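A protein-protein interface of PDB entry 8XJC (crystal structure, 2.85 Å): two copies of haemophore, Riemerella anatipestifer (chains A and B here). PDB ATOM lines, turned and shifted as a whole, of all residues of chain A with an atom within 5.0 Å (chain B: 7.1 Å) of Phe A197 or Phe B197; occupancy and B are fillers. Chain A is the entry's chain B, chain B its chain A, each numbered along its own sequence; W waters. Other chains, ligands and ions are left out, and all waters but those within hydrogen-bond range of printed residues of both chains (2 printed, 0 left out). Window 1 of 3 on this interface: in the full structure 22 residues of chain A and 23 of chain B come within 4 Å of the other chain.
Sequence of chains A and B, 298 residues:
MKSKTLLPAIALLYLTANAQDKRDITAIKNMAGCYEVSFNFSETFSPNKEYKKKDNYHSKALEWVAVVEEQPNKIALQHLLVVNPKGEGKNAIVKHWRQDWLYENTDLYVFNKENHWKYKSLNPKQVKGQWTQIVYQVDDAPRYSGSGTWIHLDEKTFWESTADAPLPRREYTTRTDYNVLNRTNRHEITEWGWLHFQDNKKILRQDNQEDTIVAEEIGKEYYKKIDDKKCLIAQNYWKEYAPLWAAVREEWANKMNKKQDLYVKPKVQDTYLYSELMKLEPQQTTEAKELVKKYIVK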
ATOM      1  N   THR A 184      -6.784  -6.027  16.712  1.00  0.00           N
ATOM      2  CA  THR A 184      -7.438  -6.801  17.736  1.00  0.00           C
ATOM      3  C   THR A 184      -6.803  -8.135  17.511  1.00  0.00           C
ATOM      4  O   THR A 184      -7.081  -8.797  16.536  1.00  0.00           O
ATOM      5  CB  THR A 184      -8.957  -6.852  17.617  1.00  0.00           C
ATOM      6  OG1 THR A 184      -9.497  -5.564  17.904  1.00  0.00           O
ATOM      7  CG2 THR A 184      -9.526  -7.844  18.605  1.00  0.00           C
ATOM      8  N   ASN A 185      -5.926  -8.529  18.411  1.00  0.00           N
ATOM      9  CA  ASN A 185      -5.171  -9.743  18.250  1.00  0.00           C
ATOM     10  C   ASN A 185      -5.668 -10.910  19.046  1.00  0.00           C
ATOM     11  O   ASN A 185      -5.966 -10.771  20.204  1.00  0.00           O
ATOM     12  CB  ASN A 185      -3.741  -9.452  18.686  1.00  0.00           C
ATOM     13  CG  ASN A 185      -3.092  -8.364  17.889  1.00  0.00           C
ATOM     14  OD1 ASN A 185      -2.988  -8.449  16.676  1.00  0.00           O
ATOM     15  ND2 ASN A 185      -2.621  -7.343  18.575  1.00  0.00           N
ATOM     16  N   ARG A 186      -5.741 -12.072  18.427  1.00  0.00           N
ATOM     17  CA  ARG A 186      -6.132 -13.279  19.128  1.00  0.00           C
ATOM     18  C   ARG A 186      -5.098 -14.346  18.991  1.00  0.00           C
ATOM     19  O   ARG A 186      -4.708 -14.690  17.903  1.00  0.00           O
ATOM     20  CB  ARG A 186      -7.477 -13.797  18.633  1.00  0.00           C
ATOM     21  CG  ARG A 186      -7.992 -15.081  19.247  1.00  0.00           C
ATOM     22  CD  ARG A 186      -9.274 -15.451  18.532  1.00  0.00           C
ATOM     23  NE  ARG A 186      -9.827 -16.734  18.937  1.00  0.00           N
ATOM     24  CZ  ARG A 186     -10.913 -16.880  19.683  1.00  0.00           C
ATOM     25  NH1 ARG A 186     -11.574 -15.822  20.111  1.00  0.00           N
ATOM     26  NH2 ARG A 186     -11.341 -18.090  19.994  1.00  0.00           N
ATOM     27  N   LEU A 195      -2.567 -20.159  16.225  1.00  0.00           N
ATOM     28  CA  LEU A 195      -3.079 -19.187  15.281  1.00  0.00           C
ATOM     29  C   LEU A 195      -3.079 -17.790  15.831  1.00  0.00           C
ATOM     30  O   LEU A 195      -3.474 -17.582  16.954  1.00  0.00           O
ATOM     31  CB  LEU A 195      -4.490 -19.566  14.834  1.00  0.00           C
ATOM     32  CG  LEU A 195      -5.383 -18.629  14.031  1.00  0.00           C
ATOM     33  CD1 LEU A 195      -4.936 -18.533  12.590  1.00  0.00           C
ATOM     34  CD2 LEU A 195      -6.802 -19.151  14.094  1.00  0.00           C
ATOM     35  N   HIS A 196      -2.609 -16.829  15.049  1.00  0.00           N
ATOM     36  CA  HIS A 196      -2.669 -15.441  15.435  1.00  0.00           C
ATOM     37  C   HIS A 196      -3.702 -14.806  14.541  1.00  0.00           C
ATOM     38  O   HIS A 196      -3.416 -14.458  13.419  1.00  0.00           O
ATOM     39  CB  HIS A 196      -1.322 -14.771  15.262  1.00  0.00           C
ATOM     40  CG  HIS A 196      -1.279 -13.344  15.713  1.00  0.00           C
ATOM     41  ND1 HIS A 196      -0.244 -12.500  15.386  1.00  0.00           N
ATOM     42  CD2 HIS A 196      -2.132 -12.616  16.466  1.00  0.00           C
ATOM     43  CE1 HIS A 196      -0.458 -11.314  15.919  1.00  0.00           C
ATOM     44  NE2 HIS A 196      -1.600 -11.356  16.576  1.00  0.00           N
ATOM     45  N   PHE A 197      -4.914 -14.664  15.039  1.00  0.00           N
ATOM     46  CA  PHE A 197      -5.976 -14.041  14.291  1.00  0.00           C
ATOM     47  C   PHE A 197      -5.983 -12.563  14.519  1.00  0.00           C
ATOM     48  O   PHE A 197      -5.811 -12.105  15.620  1.00  0.00           O
ATOM     49  CB  PHE A 197      -7.302 -14.656  14.716  1.00  0.00           C
ATOM     50  CG  PHE A 197      -8.510 -14.022  14.100  1.00  0.00           C
ATOM     51  CD1 PHE A 197      -8.953 -14.423  12.858  1.00  0.00           C
ATOM     52  CD2 PHE A 197      -9.224 -13.055  14.783  1.00  0.00           C
ATOM     53  CE1 PHE A 197     -10.070 -13.851  12.292  1.00  0.00           C
ATOM     54  CE2 PHE A 197     -10.340 -12.476  14.221  1.00  0.00           C
ATOM     55  CZ  PHE A 197     -10.764 -12.878  12.974  1.00  0.00           C
ATOM     56  N   GLN A 198      -6.193 -11.802  13.468  1.00  0.00           N
ATOM     57  CA  GLN A 198      -6.236 -10.363  13.588  1.00  0.00           C
ATOM     58  C   GLN A 198      -7.404  -9.685  12.912  1.00  0.00           C
ATOM     59  O   GLN A 198      -7.666  -9.941  11.767  1.00  0.00           O
ATOM     60  CB  GLN A 198      -4.944  -9.768  13.050  1.00  0.00           C
ATOM     61  CG  GLN A 198      -3.659 -10.283  13.660  1.00  0.00           C
ATOM     62  CD  GLN A 198      -2.449  -9.853  12.867  1.00  0.00           C
ATOM     63  OE1 GLN A 198      -1.367 -10.399  13.018  1.00  0.00           O
ATOM     64  NE2 GLN A 198      -2.634  -8.877  12.008  1.00  0.00           N
ATOM     65  N   ASP A 199      -8.125  -8.836  13.629  1.00  0.00           N
ATOM     66  CA  ASP A 199      -9.189  -8.029  13.039  1.00  0.00           C
ATOM     67  C   ASP A 199      -8.658  -6.637  13.172  1.00  0.00           C
ATOM     68  O   ASP A 199      -8.691  -6.059  14.245  1.00  0.00           O
ATOM     69  CB  ASP A 199     -10.484  -8.169  13.800  1.00  0.00           C
ATOM     70  CG  ASP A 199     -11.635  -7.474  13.130  1.00  0.00           C
ATOM     71  OD1 ASP A 199     -11.484  -7.025  11.979  1.00  0.00           O
ATOM     72  OD2 ASP A 199     -12.701  -7.380  13.763  1.00  0.00           O
ATOM     73  N   ILE A 218      -8.684  -8.533   7.676  1.00  0.00           N
ATOM     74  CA  ILE A 218      -8.737  -9.696   8.524  1.00  0.00           C
ATOM     75  C   ILE A 218      -7.469 -10.440   8.246  1.00  0.00           C
ATOM     76  O   ILE A 218      -7.060 -10.554   7.118  1.00  0.00           O
ATOM     77  CB  ILE A 218      -9.963 -10.571   8.240  1.00  0.00           C
ATOM     78  CG1 ILE A 218     -11.205  -9.953   8.865  1.00  0.00           C
ATOM     79  CG2 ILE A 218      -9.798 -11.970   8.800  1.00  0.00           C
ATOM     80  CD1 ILE A 218     -11.247 -10.082  10.365  1.00  0.00           C
ATOM     81  N   GLY A 219      -6.825 -10.923   9.282  1.00  0.00           N
ATOM     82  CA  GLY A 219      -5.630 -11.698   9.105  1.00  0.00           C
ATOM     83  C   GLY A 219      -5.618 -12.981   9.857  1.00  0.00           C
ATOM     84  O   GLY A 219      -6.045 -13.035  10.988  1.00  0.00           O
ATOM     85  N   LYS A 220      -5.128 -14.025   9.227  1.00  0.00           N
ATOM     86  CA  LYS A 220      -5.048 -15.316   9.853  1.00  0.00           C
ATOM     87  C   LYS A 220      -3.667 -15.836   9.667  1.00  0.00           C
ATOM     88  O   LYS A 220      -3.275 -16.176   8.574  1.00  0.00           O
ATOM     89  CB  LYS A 220      -6.057 -16.249   9.243  1.00  0.00           C
ATOM     90  CG  LYS A 220      -7.488 -15.945   9.622  1.00  0.00           C
ATOM     91  CD  LYS A 220      -8.414 -17.043   9.153  1.00  0.00           C
ATOM     92  CE  LYS A 220      -9.835 -16.758   9.576  1.00  0.00           C
ATOM     93  NZ  LYS A 220     -10.734 -17.875   9.208  1.00  0.00           N
ATOM     94  N   GLU A 221      -2.900 -15.861  10.744  1.00  0.00           N
ATOM     95  CA  GLU A 221      -1.529 -16.307  10.674  1.00  0.00           C
ATOM     96  C   GLU A 221      -1.413 -17.664  11.275  1.00  0.00           C
ATOM     97  O   GLU A 221      -1.684 -17.849  12.436  1.00  0.00           O
ATOM     98  CB  GLU A 221      -0.606 -15.330  11.381  1.00  0.00           C
ATOM     99  CG  GLU A 221      -1.010 -13.870  11.302  1.00  0.00           C
ATOM    100  CD  GLU A 221      -1.209 -13.377   9.889  1.00  0.00           C
ATOM    101  OE1 GLU A 221      -0.352 -13.628   9.033  1.00  0.00           O
ATOM    102  OE2 GLU A 221      -2.234 -12.726   9.639  1.00  0.00           O
ATOM    103  N   PHE B  45     -10.710 -15.340   2.264  1.00  0.00           N
ATOM    104  CA  PHE B  45      -9.749 -16.281   1.722  1.00  0.00           C
ATOM    105  C   PHE B  45     -10.329 -17.504   1.039  1.00  0.00           C
ATOM    106  O   PHE B  45     -11.430 -17.902   1.336  1.00  0.00           O
ATOM    107  CB  PHE B  45      -8.881 -16.796   2.845  1.00  0.00           C
ATOM    108  CG  PHE B  45      -8.261 -15.736   3.694  1.00  0.00           C
ATOM    109  CD1 PHE B  45      -7.225 -14.967   3.214  1.00  0.00           C
ATOM    110  CD2 PHE B  45      -8.683 -15.548   4.995  1.00  0.00           C
ATOM    111  CE1 PHE B  45      -6.647 -14.005   4.001  1.00  0.00           C
ATOM    112  CE2 PHE B  45      -8.108 -14.585   5.789  1.00  0.00           C
ATOM    113  CZ  PHE B  45      -7.087 -13.813   5.291  1.00  0.00           C
ATOM    114  N   TRP B 159     -19.936 -14.637  23.797  1.00  0.00           N
ATOM    115  CA  TRP B 159     -20.202 -16.055  23.657  1.00  0.00           C
ATOM    116  C   TRP B 159     -19.815 -16.463  22.263  1.00  0.00           C
ATOM    117  O   TRP B 159     -20.170 -15.793  21.324  1.00  0.00           O
ATOM    118  CB  TRP B 159     -21.685 -16.294  23.785  1.00  0.00           C
ATOM    119  CG  TRP B 159     -22.154 -17.697  23.650  1.00  0.00           C
ATOM    120  CD1 TRP B 159     -22.215 -18.628  24.629  1.00  0.00           C
ATOM    121  CD2 TRP B 159     -22.680 -18.316  22.473  1.00  0.00           C
ATOM    122  NE1 TRP B 159     -22.728 -19.796  24.139  1.00  0.00           N
ATOM    123  CE2 TRP B 159     -23.016 -19.632  22.813  1.00  0.00           C
ATOM    124  CE3 TRP B 159     -22.888 -17.887  21.160  1.00  0.00           C
ATOM    125  CZ2 TRP B 159     -23.553 -20.520  21.898  1.00  0.00           C
ATOM    126  CZ3 TRP B 159     -23.411 -18.770  20.255  1.00  0.00           C
ATOM    127  CH2 TRP B 159     -23.743 -20.071  20.626  1.00  0.00           C
ATOM    128  N   GLU B 160     -19.130 -17.585  22.114  1.00  0.00           N
ATOM    129  CA  GLU B 160     -18.745 -18.074  20.809  1.00  0.00           C
ATOM    130  C   GLU B 160     -18.981 -19.556  20.615  1.00  0.00           C
ATOM    131  O   GLU B 160     -18.812 -20.329  21.533  1.00  0.00           O
ATOM    132  CB  GLU B 160     -17.275 -17.744  20.597  1.00  0.00           C
ATOM    133  CG  GLU B 160     -16.795 -17.615  19.171  1.00  0.00           C
ATOM    134  CD  GLU B 160     -15.399 -17.048  19.135  1.00  0.00           C
ATOM    135  OE1 GLU B 160     -14.853 -16.793  20.227  1.00  0.00           O
ATOM    136  OE2 GLU B 160     -14.849 -16.853  18.031  1.00  0.00           O
ATOM    137  N   THR B 184     -18.735 -19.741  12.667  1.00  0.00           N
ATOM    138  CA  THR B 184     -18.227 -19.555  13.998  1.00  0.00           C
ATOM    139  C   THR B 184     -18.912 -18.271  14.369  1.00  0.00           C
ATOM    140  O   THR B 184     -18.668 -17.244  13.765  1.00  0.00           O
ATOM    141  CB  THR B 184     -16.710 -19.461  14.072  1.00  0.00           C
ATOM    142  OG1 THR B 184     -16.136 -20.723  13.735  1.00  0.00           O
ATOM    143  CG2 THR B 184     -16.274 -19.088  15.467  1.00  0.00           C
ATOM    144  N   ASN B 185     -19.800 -18.326  15.348  1.00  0.00           N
ATOM    145  CA  ASN B 185     -20.592 -17.184  15.731  1.00  0.00           C
ATOM    146  C   ASN B 185     -20.197 -16.573  17.051  1.00  0.00           C
ATOM    147  O   ASN B 185     -20.029 -17.270  18.011  1.00  0.00           O
ATOM    148  CB  ASN B 185     -22.040 -17.632  15.808  1.00  0.00           C
ATOM    149  CG  ASN B 185     -22.571 -18.150  14.501  1.00  0.00           C
ATOM    150  OD1 ASN B 185     -23.066 -19.268  14.431  1.00  0.00           O
ATOM    151  ND2 ASN B 185     -22.486 -17.340  13.464  1.00  0.00           N
ATOM    152  N   ARG B 186     -20.043 -15.257  17.090  1.00  0.00           N
ATOM    153  CA  ARG B 186     -19.699 -14.555  18.310  1.00  0.00           C
ATOM    154  C   ARG B 186     -20.730 -13.539  18.638  1.00  0.00           C
ATOM    155  O   ARG B 186     -21.024 -12.676  17.847  1.00  0.00           O
ATOM    156  CB  ARG B 186     -18.366 -13.854  18.192  1.00  0.00           C
ATOM    157  CG  ARG B 186     -17.855 -13.199  19.456  1.00  0.00           C
ATOM    158  CD  ARG B 186     -16.616 -12.402  19.115  1.00  0.00           C
ATOM    159  NE  ARG B 186     -16.139 -11.565  20.206  1.00  0.00           N
ATOM    160  CZ  ARG B 186     -15.091 -11.855  20.960  1.00  0.00           C
ATOM    161  NH1 ARG B 186     -14.406 -12.963  20.750  1.00  0.00           N
ATOM    162  NH2 ARG B 186     -14.726 -11.029  21.919  1.00  0.00           N
ATOM    163  N   HIS B 187     -21.295 -13.650  19.824  1.00  0.00           N
ATOM    164  CA  HIS B 187     -22.269 -12.715  20.257  1.00  0.00           C
ATOM    165  C   HIS B 187     -21.637 -11.907  21.340  1.00  0.00           C
ATOM    166  O   HIS B 187     -21.217 -12.437  22.329  1.00  0.00           O
ATOM    167  CB  HIS B 187     -23.490 -13.458  20.752  1.00  0.00           C
ATOM    168  CG  HIS B 187     -24.375 -13.964  19.662  1.00  0.00           C
ATOM    169  ND1 HIS B 187     -24.153 -15.157  19.017  1.00  0.00           N
ATOM    170  CD2 HIS B 187     -25.488 -13.437  19.104  1.00  0.00           C
ATOM    171  CE1 HIS B 187     -25.089 -15.343  18.105  1.00  0.00           C
ATOM    172  NE2 HIS B 187     -25.911 -14.312  18.138  1.00  0.00           N
ATOM    173  N   GLU B 188     -21.517 -10.617  21.123  1.00  0.00           N
ATOM    174  CA  GLU B 188     -20.916  -9.757  22.100  1.00  0.00           C
ATOM    175  C   GLU B 188     -21.784  -8.601  22.482  1.00  0.00           C
ATOM    176  O   GLU B 188     -22.318  -7.928  21.631  1.00  0.00           O
ATOM    177  CB  GLU B 188     -19.576  -9.234  21.611  1.00  0.00           C
ATOM    178  CG  GLU B 188     -18.826  -8.427  22.648  1.00  0.00           C
ATOM    179  CD  GLU B 188     -17.385  -8.192  22.280  1.00  0.00           C
ATOM    180  OE1 GLU B 188     -16.861  -8.926  21.425  1.00  0.00           O
ATOM    181  OE2 GLU B 188     -16.774  -7.276  22.859  1.00  0.00           O
ATOM    182  N   LEU B 195     -23.297  -7.176  19.028  1.00  0.00           N
ATOM    183  CA  LEU B 195     -22.690  -7.456  17.747  1.00  0.00           C
ATOM    184  C   LEU B 195     -22.706  -8.916  17.444  1.00  0.00           C
ATOM    185  O   LEU B 195     -22.522  -9.719  18.327  1.00  0.00           O
ATOM    186  CB  LEU B 195     -21.233  -6.969  17.759  1.00  0.00           C
ATOM    187  CG  LEU B 195     -20.189  -7.393  16.736  1.00  0.00           C
ATOM    188  CD1 LEU B 195     -20.346  -6.633  15.430  1.00  0.00           C
ATOM    189  CD2 LEU B 195     -18.823  -7.131  17.334  1.00  0.00           C
ATOM    190  N   HIS B 196     -22.956  -9.270  16.197  1.00  0.00           N
ATOM    191  CA  HIS B 196     -22.874 -10.651  15.778  1.00  0.00           C
ATOM    192  C   HIS B 196     -21.742 -10.775  14.799  1.00  0.00           C
ATOM    193  O   HIS B 196     -21.914 -10.511  13.633  1.00  0.00           O
ATOM    194  CB  HIS B 196     -24.178 -11.133  15.165  1.00  0.00           C
ATOM    195  CG  HIS B 196     -24.261 -12.614  14.985  1.00  0.00           C
ATOM    196  ND1 HIS B 196     -25.296 -13.220  14.309  1.00  0.00           N
ATOM    197  CD2 HIS B 196     -23.443 -13.612  15.392  1.00  0.00           C
ATOM    198  CE1 HIS B 196     -25.111 -14.526  14.306  1.00  0.00           C
ATOM    199  NE2 HIS B 196     -23.995 -14.789  14.956  1.00  0.00           N
ATOM    200  N   PHE B 197     -20.577 -11.167  15.282  1.00  0.00           N
ATOM    201  CA  PHE B 197     -19.418 -11.374  14.444  1.00  0.00           C
ATOM    202  C   PHE B 197     -19.390 -12.785  13.922  1.00  0.00           C
ATOM    203  O   PHE B 197     -19.593 -13.728  14.653  1.00  0.00           O
ATOM    204  CB  PHE B 197     -18.153 -11.069  15.238  1.00  0.00           C
ATOM    205  CG  PHE B 197     -16.877 -11.352  14.498  1.00  0.00           C
ATOM    206  CD1 PHE B 197     -16.354 -10.424  13.620  1.00  0.00           C
ATOM    207  CD2 PHE B 197     -16.189 -12.536  14.697  1.00  0.00           C
ATOM    208  CE1 PHE B 197     -15.182 -10.676  12.942  1.00  0.00           C
ATOM    209  CE2 PHE B 197     -15.019 -12.794  14.017  1.00  0.00           C
ATOM    210  CZ  PHE B 197     -14.514 -11.860  13.143  1.00  0.00           C
ATOM    211  N   GLN B 198     -19.126 -12.927  12.639  1.00  0.00           N
ATOM    212  CA  GLN B 198     -19.125 -14.234  12.029  1.00  0.00           C
ATOM    213  C   GLN B 198     -17.907 -14.593  11.223  1.00  0.00           C
ATOM    214  O   GLN B 198     -17.558 -13.900  10.304  1.00  0.00           O
ATOM    215  CB  GLN B 198     -20.373 -14.402  11.177  1.00  0.00           C
ATOM    216  CG  GLN B 198     -21.682 -14.258  11.924  1.00  0.00           C
ATOM    217  CD  GLN B 198     -22.876 -14.236  11.006  1.00  0.00           C
ATOM    218  OE1 GLN B 198     -23.864 -13.572  11.279  1.00  0.00           O
ATOM    219  NE2 GLN B 198     -22.785 -14.952   9.906  1.00  0.00           N
ATOM    220  N   ASP B 199     -17.243 -15.676  11.593  1.00  0.00           N
ATOM    221  CA  ASP B 199     -16.121 -16.199  10.834  1.00  0.00           C
ATOM    222  C   ASP B 199     -16.667 -17.463  10.204  1.00  0.00           C
ATOM    223  O   ASP B 199     -16.761 -18.491  10.846  1.00  0.00           O
ATOM    224  CB  ASP B 199     -14.946 -16.490  11.750  1.00  0.00           C
ATOM    225  CG  ASP B 199     -13.671 -16.774  10.997  1.00  0.00           C
ATOM    226  OD1 ASP B 199     -13.584 -16.423   9.806  1.00  0.00           O
ATOM    227  OD2 ASP B 199     -12.749 -17.351  11.602  1.00  0.00           O
ATOM    228  N   ASN B 200     -17.031 -17.394   8.937  1.00  0.00           N
ATOM    229  CA  ASN B 200     -17.670 -18.513   8.284  1.00  0.00           C
ATOM    230  C   ASN B 200     -16.912 -19.156   7.138  1.00  0.00           C
ATOM    231  O   ASN B 200     -16.143 -18.509   6.461  1.00  0.00           O
ATOM    232  CB  ASN B 200     -19.025 -18.072   7.756  1.00  0.00           C
ATOM    233  CG  ASN B 200     -19.889 -17.403   8.786  1.00  0.00           C
ATOM    234  OD1 ASN B 200     -19.735 -17.604   9.980  1.00  0.00           O
ATOM    235  ND2 ASN B 200     -20.831 -16.613   8.315  1.00  0.00           N
ATOM    236  N   GLU B 217     -15.659 -16.255   4.662  1.00  0.00           N
ATOM    237  CA  GLU B 217     -16.261 -14.950   4.797  1.00  0.00           C
ATOM    238  C   GLU B 217     -16.272 -14.423   6.187  1.00  0.00           C
ATOM    239  O   GLU B 217     -16.280 -15.168   7.143  1.00  0.00           O
ATOM    240  CB  GLU B 217     -17.680 -14.913   4.249  1.00  0.00           C
ATOM    241  CG  GLU B 217     -18.742 -15.559   5.114  1.00  0.00           C
ATOM    242  CD  GLU B 217     -20.136 -15.280   4.604  1.00  0.00           C
ATOM    243  OE1 GLU B 217     -20.261 -14.517   3.627  1.00  0.00           O
ATOM    244  OE2 GLU B 217     -21.101 -15.821   5.174  1.00  0.00           O
ATOM    245  N   ILE B 218     -16.246 -13.111   6.297  1.00  0.00           N
ATOM    246  CA  ILE B 218     -16.293 -12.468   7.584  1.00  0.00           C
ATOM    247  C   ILE B 218     -17.519 -11.604   7.598  1.00  0.00           C
ATOM    248  O   ILE B 218     -17.775 -10.864   6.675  1.00  0.00           O
ATOM    249  CB  ILE B 218     -15.027 -11.637   7.858  1.00  0.00           C
ATOM    250  CG1 ILE B 218     -13.890 -12.542   8.303  1.00  0.00           C
ATOM    251  CG2 ILE B 218     -15.270 -10.588   8.930  1.00  0.00           C
ATOM    252  CD1 ILE B 218     -14.047 -13.055   9.710  1.00  0.00           C
ATOM    253  N   GLY B 219     -18.302 -11.719   8.644  1.00  0.00           N
ATOM    254  CA  GLY B 219     -19.490 -10.927   8.763  1.00  0.00           C
ATOM    255  C   GLY B 219     -19.605 -10.225  10.065  1.00  0.00           C
ATOM    256  O   GLY B 219     -19.303 -10.770  11.092  1.00  0.00           O
ATOM    257  N   LYS B 220     -20.076  -9.003  10.022  1.00  0.00           N
ATOM    258  CA  LYS B 220     -20.209  -8.210  11.216  1.00  0.00           C
ATOM    259  C   LYS B 220     -21.552  -7.556  11.225  1.00  0.00           C
ATOM    260  O   LYS B 220     -21.834  -6.712  10.404  1.00  0.00           O
ATOM    261  CB  LYS B 220     -19.138  -7.145  11.235  1.00  0.00           C
ATOM    262  CG  LYS B 220     -17.743  -7.628  11.551  1.00  0.00           C
ATOM    263  CD  LYS B 220     -16.839  -6.434  11.743  1.00  0.00           C
ATOM    264  CE  LYS B 220     -15.390  -6.843  11.843  1.00  0.00           C
ATOM    265  NZ  LYS B 220     -14.535  -5.640  11.995  1.00  0.00           N
ATOM    266  N   GLU B 221     -22.398  -7.968  12.143  1.00  0.00           N
ATOM    267  CA  GLU B 221     -23.725  -7.415  12.238  1.00  0.00           C
ATOM    268  C   GLU B 221     -23.844  -6.549  13.453  1.00  0.00           C
ATOM    269  O   GLU B 221     -23.611  -6.991  14.551  1.00  0.00           O
ATOM    270  CB  GLU B 221     -24.751  -8.514  12.290  1.00  0.00           C
ATOM    271  CG  GLU B 221     -24.718  -9.486  11.134  1.00  0.00           C
ATOM    272  CD  GLU B 221     -25.737 -10.586  11.310  1.00  0.00           C
ATOM    273  OE1 GLU B 221     -26.442 -10.580  12.336  1.00  0.00           O
ATOM    274  OE2 GLU B 221     -25.838 -11.456  10.429  1.00  0.00           O
HETATM  275  O   HOH W   1     -12.598  -6.435   9.641  1.00  0.00           O
HETATM  276  O   HOH W   2     -13.554 -18.980   8.538  1.00  0.00           O
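The side-chain amino group (NZ) of Lys B220 lies within salt-bridge range of the side-chain carboxylate (OD2) of Asp A199.
The side-chain carboxylate of Glu B160 lies within salt-bridge range of the guanidinium group of Arg A186 (3.4 Å).
The side-chain amino group of Lys A220 lies within salt-bridge range of the side-chain carboxylate of Asp B199, at 3.2 Å.
The backbone NH (N) of Asp A199 is in hydrogen-bond range of the backbone carbonyl oxygen (O) of Thr A184 (3.1 Å).
The backbone NH (N) of Arg B186 sits at hydrogen-bond distance from the backbone carbonyl oxygen (O) of Phe B197.
The guanidinium group of Arg B186 lies within salt-bridge range of the side-chain carboxylate of Glu B160 (3.9 Å).
The backbone NH of Arg A186 lies within hydrogen-bond range of the backbone carbonyl oxygen of Phe A197, at 2.8 Å.
O of Asp B199 lies within hydrogen-bond range of N of Thr B184 (3.0 Å).
Phe A197 touches Phe B197.
Ile A218 touches Phe B45 (O to CZ, 3.7 Å).
Ile A218 touches Ile B218 (CG1 to CG1, 3.8 Å).
Phe A197 touches one residue of chain B.
Of the printed residues of chain A, Phe B197 touches Phe A197 (3.9 Å).
Printed residues of chain A within 4 Å of Phe B45: Ile A218 (3.7 Å).
Of the printed residues of chain A, Glu B160 touches Arg A186 (3.4 Å).
His B187 touches none of the printed residues of chain A.
Glu B217 touches none of the printed residues of chain A.
The nearest residue of chain B that does not touch Phe A197 is Asp B199 (4.5 Å).
The nearest printed residue of chain A that does not touch Asp B199 is Phe A197 (4.5 Å).
Of the 19 printed residues of chain B, 6 touch a printed residue of chain A.
Hydrophobic or aromatic side chains of chain B within 4 Å of the printed part of chain A: Phe B45, Phe B197 and Ile B218.
Hydrophobic or aromatic side chains of chain A within 4 Å of the printed part of chain B: Phe A197 and Ile A218.
Among the printed residues, 6 pairs touch across the chains.
Among the printed residues, Asp or Glu carboxylates within 4 Å of a Lys or Arg side-chain nitrogen of the other chain: Arg A186 with Glu B160 (3.4 Å), Asp A199 with Lys B220 (3.1 Å) and Lys A220 with Asp B199 (3.2 Å).
Phe B197 touches its own counterpart, Phe A197.
Asp A199 touches Lys B220, and with the chains exchanged Lys A220 touches Asp B199.
Ile B218 touches its own counterpart, Ile A218.
12 positions are printed for both chains.
Of the 6 pairs that touch across the chains among the printed residues, 4 have their exchanged pair printed and touching as well.
Water W1 bridges the side-chain carboxylate of Asp A199 (2.7 Å) and the side-chain amino group of Lys B220 (3.2 Å).
Water W2 lies within hydrogen-bond range of the side-chain carboxylate (OD1) of Asp B199 (2.9 Å), the side-chain amino group (NZ) of Lys A220 (3.1 Å) and the backbone carbonyl oxygen (O) of Asn B200 (3.4 Å).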
